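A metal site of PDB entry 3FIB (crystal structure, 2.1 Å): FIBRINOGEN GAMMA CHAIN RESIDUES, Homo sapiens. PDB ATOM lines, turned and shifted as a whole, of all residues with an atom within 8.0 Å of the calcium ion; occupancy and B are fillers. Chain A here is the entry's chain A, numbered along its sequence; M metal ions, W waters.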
ATOM      1  N   SER A 170     -18.600  -7.250  24.460  1.00  0.00           N
ATOM      2  CA  SER A 170     -18.552  -8.539  25.178  1.00  0.00           C
ATOM      3  C   SER A 170     -17.922  -9.685  24.363  1.00  0.00           C
ATOM      4  O   SER A 170     -18.122  -9.784  23.157  1.00  0.00           O
ATOM      5  CB  SER A 170     -19.965  -9.024  25.572  1.00  0.00           C
ATOM      6  OG  SER A 170     -20.493  -8.309  26.665  1.00  0.00           O
ATOM      7  N   ASN A 174     -15.552 -12.206  28.981  1.00  0.00           N
ATOM      8  CA  ASN A 174     -15.672 -10.855  29.510  1.00  0.00           C
ATOM      9  C   ASN A 174     -17.077 -10.403  29.131  1.00  0.00           C
ATOM     10  O   ASN A 174     -17.304  -9.800  28.088  1.00  0.00           O
ATOM     11  CB  ASN A 174     -14.618  -9.933  28.889  1.00  0.00           C
ATOM     12  CG  ASN A 174     -14.306  -8.725  29.756  1.00  0.00           C
ATOM     13  OD1 ASN A 174     -15.172  -7.902  30.024  1.00  0.00           O
ATOM     14  ND2 ASN A 174     -13.058  -8.603  30.180  1.00  0.00           N
ATOM     15  N   ASP A 175     -18.009 -10.782  29.985  1.00  0.00           N
ATOM     16  CA  ASP A 175     -19.430 -10.500  29.821  1.00  0.00           C
ATOM     17  C   ASP A 175     -19.791  -9.107  30.340  1.00  0.00           C
ATOM     18  O   ASP A 175     -19.696  -8.849  31.532  1.00  0.00           O
ATOM     19  CB  ASP A 175     -20.196 -11.598  30.571  1.00  0.00           C
ATOM     20  CG  ASP A 175     -21.691 -11.459  30.449  1.00  0.00           C
ATOM     21  OD1 ASP A 175     -22.196 -10.399  30.021  1.00  0.00           O
ATOM     22  OD2 ASP A 175     -22.390 -12.428  30.787  1.00  0.00           O
ATOM     23  N   ASN A 176     -20.268  -8.242  29.443  1.00  0.00           N
ATOM     24  CA  ASN A 176     -20.658  -6.871  29.805  1.00  0.00           C
ATOM     25  C   ASN A 176     -21.978  -6.512  29.168  1.00  0.00           C
ATOM     26  O   ASN A 176     -22.271  -5.349  28.932  1.00  0.00           O
ATOM     27  CB  ASN A 176     -19.589  -5.867  29.323  1.00  0.00           C
ATOM     28  CG  ASN A 176     -18.230  -6.146  29.900  1.00  0.00           C
ATOM     29  OD1 ASN A 176     -18.013  -6.006  31.116  1.00  0.00           O
ATOM     30  ND2 ASN A 176     -17.274  -6.533  29.049  1.00  0.00           N
ATOM     31  N   ASP A 177     -22.779  -7.526  28.847  1.00  0.00           N
ATOM     32  CA  ASP A 177     -24.069  -7.296  28.229  1.00  0.00           C
ATOM     33  C   ASP A 177     -25.163  -7.020  29.261  1.00  0.00           C
ATOM     34  O   ASP A 177     -24.904  -6.935  30.464  1.00  0.00           O
ATOM     35  CB  ASP A 177     -24.449  -8.477  27.301  1.00  0.00           C
ATOM     36  CG  ASP A 177     -24.615  -9.814  28.044  1.00  0.00           C
ATOM     37  OD1 ASP A 177     -25.033  -9.799  29.221  1.00  0.00           O
ATOM     38  OD2 ASP A 177     -24.354 -10.880  27.452  1.00  0.00           O
ATOM     39  N   LYS A 178     -26.399  -6.966  28.785  1.00  0.00           N
ATOM     40  CA  LYS A 178     -27.547  -6.694  29.641  1.00  0.00           C
ATOM     41  C   LYS A 178     -28.397  -7.950  29.921  1.00  0.00           C
ATOM     42  O   LYS A 178     -29.525  -7.849  30.388  1.00  0.00           O
ATOM     43  CB  LYS A 178     -28.401  -5.618  28.969  1.00  0.00           C
ATOM     44  CG  LYS A 178     -27.672  -4.294  28.796  1.00  0.00           C
ATOM     45  CD  LYS A 178     -28.024  -3.371  29.956  1.00  0.00           C
ATOM     46  CE  LYS A 178     -27.377  -2.000  29.839  1.00  0.00           C
ATOM     47  NZ  LYS A 178     -25.914  -2.016  30.161  1.00  0.00           N
ATOM     48  N   PHE A 179     -27.822  -9.123  29.659  1.00  0.00           N
ATOM     49  CA  PHE A 179     -28.478 -10.416  29.810  1.00  0.00           C
ATOM     50  C   PHE A 179     -28.035 -11.171  31.070  1.00  0.00           C
ATOM     51  O   PHE A 179     -26.873 -11.099  31.486  1.00  0.00           O
ATOM     52  CB  PHE A 179     -28.131 -11.253  28.565  1.00  0.00           C
ATOM     53  CG  PHE A 179     -28.824 -12.575  28.495  1.00  0.00           C
ATOM     54  CD1 PHE A 179     -30.127 -12.736  28.928  1.00  0.00           C
ATOM     55  CD2 PHE A 179     -28.165 -13.676  27.938  1.00  0.00           C
ATOM     56  CE1 PHE A 179     -30.764 -13.989  28.826  1.00  0.00           C
ATOM     57  CE2 PHE A 179     -28.797 -14.918  27.843  1.00  0.00           C
ATOM     58  CZ  PHE A 179     -30.086 -15.077  28.276  1.00  0.00           C
ATOM     59  N   GLU A 180     -28.985 -11.915  31.644  1.00  0.00           N
ATOM     60  CA  GLU A 180     -28.751 -12.720  32.837  1.00  0.00           C
ATOM     61  C   GLU A 180     -27.749 -13.801  32.440  1.00  0.00           C
ATOM     62  O   GLU A 180     -26.941 -14.247  33.271  1.00  0.00           O
ATOM     63  CB  GLU A 180     -30.054 -13.389  33.313  1.00  0.00           C
ATOM     64  CG  GLU A 180     -31.175 -12.436  33.726  1.00  0.00           C
ATOM     65  CD  GLU A 180     -32.244 -12.235  32.631  1.00  0.00           C
ATOM     66  OE1 GLU A 180     -31.982 -11.475  31.661  1.00  0.00           O
ATOM     67  OE2 GLU A 180     -33.344 -12.822  32.745  1.00  0.00           O
ATOM     68  N   GLY A 181     -27.823 -14.234  31.193  1.00  0.00           N
ATOM     69  CA  GLY A 181     -26.879 -15.213  30.678  1.00  0.00           C
ATOM     70  C   GLY A 181     -25.668 -14.522  30.035  1.00  0.00           C
ATOM     71  O   GLY A 181     -25.358 -13.344  30.327  1.00  0.00           O
ATOM     72  N   ASN A 182     -25.002 -15.224  29.144  1.00  0.00           N
ATOM     73  CA  ASN A 182     -23.815 -14.687  28.477  1.00  0.00           C
ATOM     74  C   ASN A 182     -24.070 -14.741  26.978  1.00  0.00           C
ATOM     75  O   ASN A 182     -23.939 -15.792  26.377  1.00  0.00           O
ATOM     76  CB  ASN A 182     -22.571 -15.512  28.857  1.00  0.00           C
ATOM     77  CG  ASN A 182     -21.250 -14.945  28.295  1.00  0.00           C
ATOM     78  OD1 ASN A 182     -21.235 -14.214  27.295  1.00  0.00           O
ATOM     79  ND2 ASN A 182     -20.137 -15.298  28.917  1.00  0.00           N
ATOM     80  N   CYS A 183     -24.458 -13.614  26.394  1.00  0.00           N
ATOM     81  CA  CYS A 183     -24.712 -13.551  24.960  1.00  0.00           C
ATOM     82  C   CYS A 183     -23.507 -13.997  24.098  1.00  0.00           C
ATOM     83  O   CYS A 183     -23.665 -14.787  23.162  1.00  0.00           O
ATOM     84  CB  CYS A 183     -25.083 -12.132  24.545  1.00  0.00           C
ATOM     85  SG  CYS A 183     -26.677 -11.524  25.168  1.00  0.00           S
ATOM     86  N   ALA A 184     -22.336 -13.451  24.390  1.00  0.00           N
ATOM     87  CA  ALA A 184     -21.137 -13.772  23.600  1.00  0.00           C
ATOM     88  C   ALA A 184     -20.782 -15.254  23.614  1.00  0.00           C
ATOM     89  O   ALA A 184     -20.325 -15.791  22.599  1.00  0.00           O
ATOM     90  CB  ALA A 184     -19.961 -12.945  24.074  1.00  0.00           C
ATOM     91  N   ASN A 194     -26.503  -6.621  23.870  1.00  0.00           N
ATOM     92  CA  ASN A 194     -27.494  -6.058  24.747  1.00  0.00           C
ATOM     93  C   ASN A 194     -28.138  -7.294  25.377  1.00  0.00           C
ATOM     94  O   ASN A 194     -27.604  -7.864  26.328  1.00  0.00           O
ATOM     95  CB  ASN A 194     -28.526  -5.239  23.957  1.00  0.00           C
ATOM     96  CG  ASN A 194     -29.485  -4.463  24.863  1.00  0.00           C
ATOM     97  OD1 ASN A 194     -29.653  -4.791  26.044  1.00  0.00           O
ATOM     98  ND2 ASN A 194     -30.103  -3.437  24.307  1.00  0.00           N
ATOM     99  N   LYS A 195     -29.229  -7.748  24.777  1.00  0.00           N
ATOM    100  CA  LYS A 195     -29.926  -8.938  25.241  1.00  0.00           C
ATOM    101  C   LYS A 195     -30.780  -9.600  24.159  1.00  0.00           C
ATOM    102  O   LYS A 195     -31.997  -9.700  24.310  1.00  0.00           O
ATOM    103  CB  LYS A 195     -30.780  -8.607  26.468  1.00  0.00           C
ATOM    104  CG  LYS A 195     -31.052  -9.838  27.242  1.00  0.00           C
ATOM    105  CD  LYS A 195     -32.487  -9.981  27.624  1.00  0.00           C
ATOM    106  CE  LYS A 195     -32.740  -9.362  28.959  1.00  0.00           C
ATOM    107  NZ  LYS A 195     -33.992  -9.984  29.437  1.00  0.00           N
HETATM  108 CA    CA M   1     -24.564 -11.260  31.205  1.00  0.00          CA
HETATM  109  O   HOH W   1     -24.081  -9.067  32.142  1.00  0.00           O
HETATM  110  O   HOH W   2     -24.369 -12.197  33.446  1.00  0.00           O
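OG of Ser 170 lies within hydrogen-bond range of N of Asp 177, 3.3 Å away. The side-chain carboxylate of Asp 177 is in hydrogen-bond range of the backbone NH of Cys 183 (2.9 Å).
Of the 14 residues printed, 4 come within 4 Å of the calcium ion.
The calcium ion is bound by O of Phe 179 (2.3 Å), O of Gly 181 (2.4 Å), water W1 (2.4 Å), water W2 (2.4 Å), OD2 of Asp 175 (2.5 Å), OD1 of Asp 177 (2.5 Å) and OD1 of Asp 175 (2.8 Å). The calcium ion has seven donor atoms within binding distance.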
